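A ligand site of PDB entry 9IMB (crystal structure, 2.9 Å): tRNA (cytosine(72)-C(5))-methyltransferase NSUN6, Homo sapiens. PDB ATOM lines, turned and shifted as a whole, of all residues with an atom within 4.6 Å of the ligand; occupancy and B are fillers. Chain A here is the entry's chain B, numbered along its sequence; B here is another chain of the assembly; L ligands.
The side-chain carboxylate of Asp 323 lies within salt-bridge range of a nitrogen (N1) of the ligand (2.5 Å).
The side-chain carboxylate (OD1) of Asp 266 is in hydrogen-bond range of an oxygen (O5) of the ligand.
N of Gly 294 lies within hydrogen-bond range of N6 of the ligand (2.9 Å).
The side-chain carboxylate of Asp 293 sits at hydrogen-bond distance from a nitrogen (N5) of the ligand, at 2.9 Å.
O of Ala 244 lies close to O4 of the ligand, at 3.4 Å.
The backbone carbonyl oxygen of Cys 242 lies within hydrogen-bond range of a nitrogen (N1) of the ligand (3.5 Å).
O4 of the ligand lies within hydrogen-bond range of NZ of Lys 271, 3.1 Å away.
N2 of the ligand is in hydrogen-bond range of O of Ala 324 (3.3 Å).
NZ of Lys 248 is in salt-bridge range of O2 of the ligand (3.4 Å).
A nitrogen (N7) of the ligand lies within hydrogen-bond range of the backbone NH (N) of Lys 267 (3.5 Å).
The side-chain carboxylate (OD2) of Asp 323 lies within salt-bridge range of the side-chain amino group (NZ) of Lys 248, 2.9 Å away.
N of Ala 244 is in hydrogen-bond range of OD2 of Asp 266, 3.0 Å away.
N of Ala 243 lies within hydrogen-bond range of OD2 of Asp 266, at 3.5 Å.
O of Asp 266 sits at hydrogen-bond distance from N of Phe 292 (3.0 Å).
OD1 of Asp 293 sits at hydrogen-bond distance from OG1 of Thr 295, 2.4 Å away.
O2 of C 12 of chain B lies within hydrogen-bond range of SG of Cys 373, at 3.3 Å.
The backbone NH (N) of Ala 243 lies within hydrogen-bond range of the backbone carbonyl oxygen (O) of Leu 265, 2.9 Å away.
Leu 241 touches the ligand.
O of Ala 243 touches C1 of the ligand (3.3 Å).
CD of Pro 245 touches O1 of the ligand (3.2 Å).
Phe 292 touches the ligand (O to N6, 3.5 Å).
Pro 325 touches the ligand (CA to C6, 3.7 Å).
C 12 of chain B touches the ligand.
Hydrophobic or aromatic side chains that line the ligand: Pro 245 and Pro 325.
The nearest printed residue that does not touch the ligand is Gly 247 (4.004 Å).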
ATOM      1  N   LEU A 241     -27.219   9.280   3.771  1.00  0.00           N
ATOM      2  CA  LEU A 241     -28.534   8.714   4.168  1.00  0.00           C
ATOM      3  C   LEU A 241     -28.821   8.987   5.641  1.00  0.00           C
ATOM      4  O   LEU A 241     -29.870   9.551   5.923  1.00  0.00           O
ATOM      5  CB  LEU A 241     -28.527   7.219   3.846  1.00  0.00           C
ATOM      6  CG  LEU A 241     -29.427   6.774   2.702  1.00  0.00           C
ATOM      7  CD1 LEU A 241     -29.629   5.269   2.732  1.00  0.00           C
ATOM      8  CD2 LEU A 241     -30.769   7.489   2.762  1.00  0.00           C
ATOM      9  N   CYS A 242     -27.979   8.512   6.535  1.00  0.00           N
ATOM     10  CA  CYS A 242     -28.116   8.812   7.977  1.00  0.00           C
ATOM     11  C   CYS A 242     -27.030   9.846   8.263  1.00  0.00           C
ATOM     12  O   CYS A 242     -25.887   9.427   8.353  1.00  0.00           O
ATOM     13  CB  CYS A 242     -28.002   7.505   8.744  1.00  0.00           C
ATOM     14  SG  CYS A 242     -28.772   6.098   7.900  1.00  0.00           S
ATOM     15  N   ALA A 243     -27.383  11.123   8.389  1.00  0.00           N
ATOM     16  CA  ALA A 243     -26.347  12.186   8.432  1.00  0.00           C
ATOM     17  C   ALA A 243     -26.222  12.993   9.726  1.00  0.00           C
ATOM     18  O   ALA A 243     -25.108  13.402  10.027  1.00  0.00           O
ATOM     19  CB  ALA A 243     -26.709  13.132   7.341  1.00  0.00           C
ATOM     20  N   ALA A 244     -27.311  13.281  10.406  1.00  0.00           N
ATOM     21  CA  ALA A 244     -27.274  14.158  11.578  1.00  0.00           C
ATOM     22  C   ALA A 244     -26.232  13.661  12.581  1.00  0.00           C
ATOM     23  O   ALA A 244     -26.090  12.451  12.783  1.00  0.00           O
ATOM     24  CB  ALA A 244     -28.651  14.217  12.241  1.00  0.00           C
ATOM     25  N   PRO A 245     -25.484  14.572  13.225  1.00  0.00           N
ATOM     26  CA  PRO A 245     -25.665  16.033  13.153  1.00  0.00           C
ATOM     27  C   PRO A 245     -25.012  16.703  11.947  1.00  0.00           C
ATOM     28  O   PRO A 245     -25.022  17.927  11.859  1.00  0.00           O
ATOM     29  CB  PRO A 245     -25.016  16.507  14.454  1.00  0.00           C
ATOM     30  CG  PRO A 245     -23.909  15.536  14.675  1.00  0.00           C
ATOM     31  CD  PRO A 245     -24.407  14.206  14.155  1.00  0.00           C
ATOM     32  N   GLY A 247     -21.636  15.993  10.764  1.00  0.00           N
ATOM     33  CA  GLY A 247     -20.191  16.145  10.780  1.00  0.00           C
ATOM     34  C   GLY A 247     -19.546  15.662   9.495  1.00  0.00           C
ATOM     35  O   GLY A 247     -18.696  16.333   8.914  1.00  0.00           O
ATOM     36  N   LYS A 248     -19.949  14.471   9.024  1.00  0.00           N
ATOM     37  CA  LYS A 248     -19.435  13.975   7.752  1.00  0.00           C
ATOM     38  C   LYS A 248     -20.043  14.715   6.574  1.00  0.00           C
ATOM     39  O   LYS A 248     -19.367  14.900   5.556  1.00  0.00           O
ATOM     40  CB  LYS A 248     -19.700  12.477   7.639  1.00  0.00           C
ATOM     41  CG  LYS A 248     -19.000  11.643   8.702  1.00  0.00           C
ATOM     42  CD  LYS A 248     -19.378  10.180   8.616  1.00  0.00           C
ATOM     43  CE  LYS A 248     -18.750   9.389   9.753  1.00  0.00           C
ATOM     44  NZ  LYS A 248     -19.200   9.885  11.078  1.00  0.00           N
ATOM     45  N   LEU A 265     -29.975  13.269   4.900  1.00  0.00           N
ATOM     46  CA  LEU A 265     -31.227  12.779   5.453  1.00  0.00           C
ATOM     47  C   LEU A 265     -31.040  12.370   6.904  1.00  0.00           C
ATOM     48  O   LEU A 265     -29.930  12.046   7.345  1.00  0.00           O
ATOM     49  CB  LEU A 265     -31.777  11.591   4.651  1.00  0.00           C
ATOM     50  CG  LEU A 265     -32.173  11.815   3.189  1.00  0.00           C
ATOM     51  CD1 LEU A 265     -32.675  10.513   2.579  1.00  0.00           C
ATOM     52  CD2 LEU A 265     -33.233  12.897   3.075  1.00  0.00           C
ATOM     53  N   ASP A 266     -32.144  12.394   7.651  1.00  0.00           N
ATOM     54  CA  ASP A 266     -32.219  11.884   9.007  1.00  0.00           C
ATOM     55  C   ASP A 266     -33.686  11.885   9.427  1.00  0.00           C
ATOM     56  O   ASP A 266     -34.454  12.742   9.002  1.00  0.00           O
ATOM     57  CB  ASP A 266     -31.379  12.698   9.991  1.00  0.00           C
ATOM     58  CG  ASP A 266     -30.817  11.852  11.123  1.00  0.00           C
ATOM     59  OD1 ASP A 266     -31.561  11.580  12.086  1.00  0.00           O
ATOM     60  OD2 ASP A 266     -29.642  11.446  11.040  1.00  0.00           O
ATOM     61  N   LYS A 267     -34.053  10.916  10.275  1.00  0.00           N
ATOM     62  CA  LYS A 267     -35.458  10.684  10.583  1.00  0.00           C
ATOM     63  C   LYS A 267     -36.005  11.580  11.697  1.00  0.00           C
ATOM     64  O   LYS A 267     -37.218  11.562  11.931  1.00  0.00           O
ATOM     65  CB  LYS A 267     -35.666   9.216  10.956  1.00  0.00           C
ATOM     66  CG  LYS A 267     -35.439   8.902  12.428  1.00  0.00           C
ATOM     67  CD  LYS A 267     -35.801   7.462  12.756  1.00  0.00           C
ATOM     68  CE  LYS A 267     -35.556   7.142  14.216  1.00  0.00           C
ATOM     69  NZ  LYS A 267     -34.478   7.990  14.805  1.00  0.00           N
ATOM     70  N   LYS A 271     -32.804  16.803  14.784  1.00  0.00           N
ATOM     71  CA  LYS A 271     -31.486  16.350  14.344  1.00  0.00           C
ATOM     72  C   LYS A 271     -31.150  16.897  12.958  1.00  0.00           C
ATOM     73  O   LYS A 271     -29.992  17.219  12.671  1.00  0.00           O
ATOM     74  CB  LYS A 271     -31.435  14.817  14.342  1.00  0.00           C
ATOM     75  CG  LYS A 271     -30.819  14.229  15.598  1.00  0.00           C
ATOM     76  CD  LYS A 271     -30.882  12.708  15.569  1.00  0.00           C
ATOM     77  CE  LYS A 271     -29.930  12.101  16.590  1.00  0.00           C
ATOM     78  NZ  LYS A 271     -28.522  12.079  16.093  1.00  0.00           N
ATOM     79  N   PHE A 292     -36.475  12.635   6.762  1.00  0.00           N
ATOM     80  CA  PHE A 292     -37.059  11.605   5.920  1.00  0.00           C
ATOM     81  C   PHE A 292     -36.517  10.249   6.334  1.00  0.00           C
ATOM     82  O   PHE A 292     -35.393  10.129   6.822  1.00  0.00           O
ATOM     83  CB  PHE A 292     -36.751  11.872   4.438  1.00  0.00           C
ATOM     84  CG  PHE A 292     -37.698  11.196   3.492  1.00  0.00           C
ATOM     85  CD1 PHE A 292     -38.885  11.805   3.129  1.00  0.00           C
ATOM     86  CD2 PHE A 292     -37.384   9.959   2.946  1.00  0.00           C
ATOM     87  CE1 PHE A 292     -39.758  11.185   2.241  1.00  0.00           C
ATOM     88  CE2 PHE A 292     -38.249   9.341   2.063  1.00  0.00           C
ATOM     89  CZ  PHE A 292     -39.432   9.954   1.713  1.00  0.00           C
ATOM     90  N   ASP A 293     -37.344   9.218   6.145  1.00  0.00           N
ATOM     91  CA  ASP A 293     -36.941   7.839   6.420  1.00  0.00           C
ATOM     92  C   ASP A 293     -36.094   7.330   5.261  1.00  0.00           C
ATOM     93  O   ASP A 293     -36.584   7.189   4.138  1.00  0.00           O
ATOM     94  CB  ASP A 293     -38.164   6.955   6.636  1.00  0.00           C
ATOM     95  CG  ASP A 293     -37.815   5.630   7.294  1.00  0.00           C
ATOM     96  OD1 ASP A 293     -36.768   5.034   6.962  1.00  0.00           O
ATOM     97  OD2 ASP A 293     -38.606   5.175   8.156  1.00  0.00           O
ATOM     98  N   GLY A 294     -34.822   7.041   5.536  1.00  0.00           N
ATOM     99  CA  GLY A 294     -33.928   6.559   4.494  1.00  0.00           C
ATOM    100  C   GLY A 294     -34.358   5.235   3.889  1.00  0.00           C
ATOM    101  O   GLY A 294     -34.106   4.972   2.716  1.00  0.00           O
ATOM    102  N   THR A 295     -35.031   4.390   4.681  1.00  0.00           N
ATOM    103  CA  THR A 295     -35.539   3.122   4.178  1.00  0.00           C
ATOM    104  C   THR A 295     -36.678   3.306   3.176  1.00  0.00           C
ATOM    105  O   THR A 295     -37.086   2.329   2.545  1.00  0.00           O
ATOM    106  CB  THR A 295     -36.009   2.243   5.337  1.00  0.00           C
ATOM    107  OG1 THR A 295     -37.141   2.851   5.975  1.00  0.00           O
ATOM    108  CG2 THR A 295     -34.893   2.067   6.358  1.00  0.00           C
ATOM    109  N   ASP A 323     -23.504   5.979   6.894  1.00  0.00           N
ATOM    110  CA  ASP A 323     -23.023   5.892   8.274  1.00  0.00           C
ATOM    111  C   ASP A 323     -24.193   5.390   9.109  1.00  0.00           C
ATOM    112  O   ASP A 323     -24.902   6.146   9.783  1.00  0.00           O
ATOM    113  CB  ASP A 323     -22.496   7.237   8.754  1.00  0.00           C
ATOM    114  CG  ASP A 323     -21.746   7.138  10.067  1.00  0.00           C
ATOM    115  OD1 ASP A 323     -21.393   6.007  10.467  1.00  0.00           O
ATOM    116  OD2 ASP A 323     -21.519   8.177  10.709  1.00  0.00           O
ATOM    117  N   ALA A 324     -24.394   4.082   9.040  1.00  0.00           N
ATOM    118  CA  ALA A 324     -25.636   3.490   9.506  1.00  0.00           C
ATOM    119  C   ALA A 324     -25.773   3.593  11.022  1.00  0.00           C
ATOM    120  O   ALA A 324     -24.775   3.650  11.743  1.00  0.00           O
ATOM    121  CB  ALA A 324     -25.722   2.031   9.085  1.00  0.00           C
ATOM    122  N   PRO A 325     -27.007   3.628  11.533  1.00  0.00           N
ATOM    123  CA  PRO A 325     -27.210   3.452  12.978  1.00  0.00           C
ATOM    124  C   PRO A 325     -26.722   2.084  13.414  1.00  0.00           C
ATOM    125  O   PRO A 325     -26.814   1.106  12.666  1.00  0.00           O
ATOM    126  CB  PRO A 325     -28.729   3.594  13.140  1.00  0.00           C
ATOM    127  CG  PRO A 325     -29.295   3.375  11.778  1.00  0.00           C
ATOM    128  CD  PRO A 325     -28.271   3.884  10.824  1.00  0.00           C
ATOM    129  N   LEU A 350     -32.370  -2.888  10.392  1.00  0.00           N
ATOM    130  CA  LEU A 350     -32.432  -1.513   9.891  1.00  0.00           C
ATOM    131  C   LEU A 350     -31.228  -1.191   9.017  1.00  0.00           C
ATOM    132  O   LEU A 350     -31.351  -0.410   8.060  1.00  0.00           O
ATOM    133  CB  LEU A 350     -32.521  -0.535  11.066  1.00  0.00           C
ATOM    134  CG  LEU A 350     -32.536   0.954  10.733  1.00  0.00           C
ATOM    135  CD1 LEU A 350     -33.698   1.288   9.802  1.00  0.00           C
ATOM    136  CD2 LEU A 350     -32.612   1.788  12.005  1.00  0.00           C
ATOM    137  N   LEU A 354     -31.576   0.121   5.051  1.00  0.00           N
ATOM    138  CA  LEU A 354     -30.916   1.314   4.538  1.00  0.00           C
ATOM    139  C   LEU A 354     -29.898   0.954   3.457  1.00  0.00           C
ATOM    140  O   LEU A 354     -29.691   1.739   2.526  1.00  0.00           O
ATOM    141  CB  LEU A 354     -30.240   2.078   5.679  1.00  0.00           C
ATOM    142  CG  LEU A 354     -31.180   2.696   6.709  1.00  0.00           C
ATOM    143  CD1 LEU A 354     -30.487   2.850   8.052  1.00  0.00           C
ATOM    144  CD2 LEU A 354     -31.699   4.039   6.214  1.00  0.00           C
ATOM    145  N   CYS A 373     -20.248   2.704  14.052  1.00  0.00           N
ATOM    146  CA  CYS A 373     -19.475   3.058  15.232  1.00  0.00           C
ATOM    147  C   CYS A 373     -19.600   1.988  16.313  1.00  0.00           C
ATOM    148  O   CYS A 373     -19.754   2.299  17.500  1.00  0.00           O
ATOM    149  CB  CYS A 373     -19.879   4.432  15.763  1.00  0.00           C
ATOM    150  SG  CYS A 373     -21.669   4.711  15.797  1.00  0.00           S
ATOM    151  P     C B  12     -20.828  10.729  20.698  1.00  0.00           P
ATOM    152  OP1   C B  12     -19.839  10.869  21.792  1.00  0.00           O
ATOM    153  OP2   C B  12     -21.889  11.760  20.518  1.00  0.00           O
ATOM    154  O5'   C B  12     -20.037  10.735  19.316  1.00  0.00           O
ATOM    155  C5'   C B  12     -18.871   9.943  19.118  1.00  0.00           C
ATOM    156  C4'   C B  12     -18.994   9.085  17.885  1.00  0.00           C
ATOM    157  O4'   C B  12     -20.171   8.244  17.998  1.00  0.00           O
ATOM    158  C3'   C B  12     -19.191   9.812  16.566  1.00  0.00           C
ATOM    159  O3'   C B  12     -17.978  10.289  16.006  1.00  0.00           O
ATOM    160  C2'   C B  12     -19.866   8.749  15.694  1.00  0.00           C
ATOM    161  O2'   C B  12     -18.900   7.858  15.151  1.00  0.00           O
ATOM    162  C1'   C B  12     -20.714   7.993  16.715  1.00  0.00           C
ATOM    163  N1    C B  12     -22.140   8.408  16.703  1.00  0.00           N
ATOM    164  C2    C B  12     -23.041   7.674  17.468  1.00  0.00           C
ATOM    165  O2    C B  12     -22.616   6.740  18.178  1.00  0.00           O
ATOM    166  N3    C B  12     -24.355   8.016  17.469  1.00  0.00           N
ATOM    167  C4    C B  12     -24.777   9.025  16.703  1.00  0.00           C
ATOM    168  N4    C B  12     -26.078   9.319  16.720  1.00  0.00           N
ATOM    169  C5    C B  12     -23.878   9.772  15.893  1.00  0.00           C
ATOM    170  C6    C B  12     -22.583   9.426  15.907  1.00  0.00           C
ATOM    171  P     U B  13     -17.681  11.864  15.943  1.00  0.00           P
ATOM    172  OP1   U B  13     -18.809  12.537  15.249  1.00  0.00           O
ATOM    173  OP2   U B  13     -16.295  12.043  15.432  1.00  0.00           O
ATOM    174  O5'   U B  13     -17.690  12.317  17.472  1.00  0.00           O
ATOM    175  C5'   U B  13     -18.288  13.537  17.886  1.00  0.00           C
ATOM    176  C4'   U B  13     -18.373  13.619  19.380  1.00  0.00           C
ATOM    177  O4'   U B  13     -17.131  13.116  19.944  1.00  0.00           O
ATOM    178  C3'   U B  13     -18.578  15.020  19.959  1.00  0.00           C
ATOM    179  O3'   U B  13     -19.418  14.969  21.104  1.00  0.00           O
ATOM    180  C2'   U B  13     -17.165  15.446  20.363  1.00  0.00           C
ATOM    181  O2'   U B  13     -17.127  16.356  21.433  1.00  0.00           O
ATOM    182  C1'   U B  13     -16.513  14.113  20.735  1.00  0.00           C
ATOM    183  N1    U B  13     -15.072  14.079  20.440  1.00  0.00           N
ATOM    184  C2    U B  13     -14.176  14.410  21.442  1.00  0.00           C
ATOM    185  O2    U B  13     -14.537  14.729  22.560  1.00  0.00           O
ATOM    186  N3    U B  13     -12.848  14.352  21.087  1.00  0.00           N
ATOM    187  C4    U B  13     -12.342  14.005  19.858  1.00  0.00           C
ATOM    188  O4    U B  13     -11.109  14.004  19.683  1.00  0.00           O
ATOM    189  C5    U B  13     -13.314  13.672  18.872  1.00  0.00           C
ATOM    190  C6    U B  13     -14.614  13.726  19.196  1.00  0.00           C
HETATM  191  N1  LIG L   1     -23.207  10.037  10.480  1.00  0.00           N
HETATM  192  C1  LIG L   1     -23.795  10.770  11.540  1.00  0.00           C
HETATM  193  C2  LIG L   1     -22.674  11.520  12.261  1.00  0.00           C
HETATM  194  O1  LIG L   1     -22.647  11.600  13.499  1.00  0.00           O
HETATM  195  O2  LIG L   1     -21.756  12.078  11.596  1.00  0.00           O
HETATM  196  C3  LIG L   1     -24.545   9.902  12.508  1.00  0.00           C
HETATM  197  C4  LIG L   1     -25.104   8.560  11.956  1.00  0.00           C
HETATM  198  C5  LIG L   1     -25.492   7.666  13.184  1.00  0.00           C
HETATM  199  N2  LIG L   1     -24.625   6.577  13.295  1.00  0.00           N
HETATM  200  C6  LIG L   1     -26.957   7.173  13.055  1.00  0.00           C
HETATM  201  C7  LIG L   1     -27.895   8.232  12.612  1.00  0.00           C
HETATM  202  O3  LIG L   1     -29.011   7.571  11.591  1.00  0.00           O
HETATM  203  C8  LIG L   1     -28.578   8.717  13.646  1.00  0.00           C
HETATM  204  O4  LIG L   1     -28.377  10.170  13.701  1.00  0.00           O
HETATM  205  C9  LIG L   1     -30.071   8.383  13.378  1.00  0.00           C
HETATM  206  O5  LIG L   1     -30.836   9.395  13.755  1.00  0.00           O
HETATM  207  C10 LIG L   1     -30.116   8.211  11.819  1.00  0.00           C
HETATM  208  N3  LIG L   1     -31.201   7.361  11.352  1.00  0.00           N
HETATM  209  C11 LIG L   1     -31.656   6.288  11.952  1.00  0.00           C
HETATM  210  N4  LIG L   1     -32.611   5.769  11.221  1.00  0.00           N
HETATM  211  C12 LIG L   1     -32.771   6.525  10.126  1.00  0.00           C
HETATM  212  C13 LIG L   1     -33.625   6.468   9.005  1.00  0.00           C
HETATM  213  N5  LIG L   1     -34.608   5.422   8.876  1.00  0.00           N
HETATM  214  N6  LIG L   1     -33.505   7.413   8.089  1.00  0.00           N
HETATM  215  C14 LIG L   1     -32.602   8.397   8.196  1.00  0.00           C
HETATM  216  N7  LIG L   1     -31.800   8.466   9.216  1.00  0.00           N
HETATM  217  C15 LIG L   1     -31.862   7.541  10.209  1.00  0.00           C
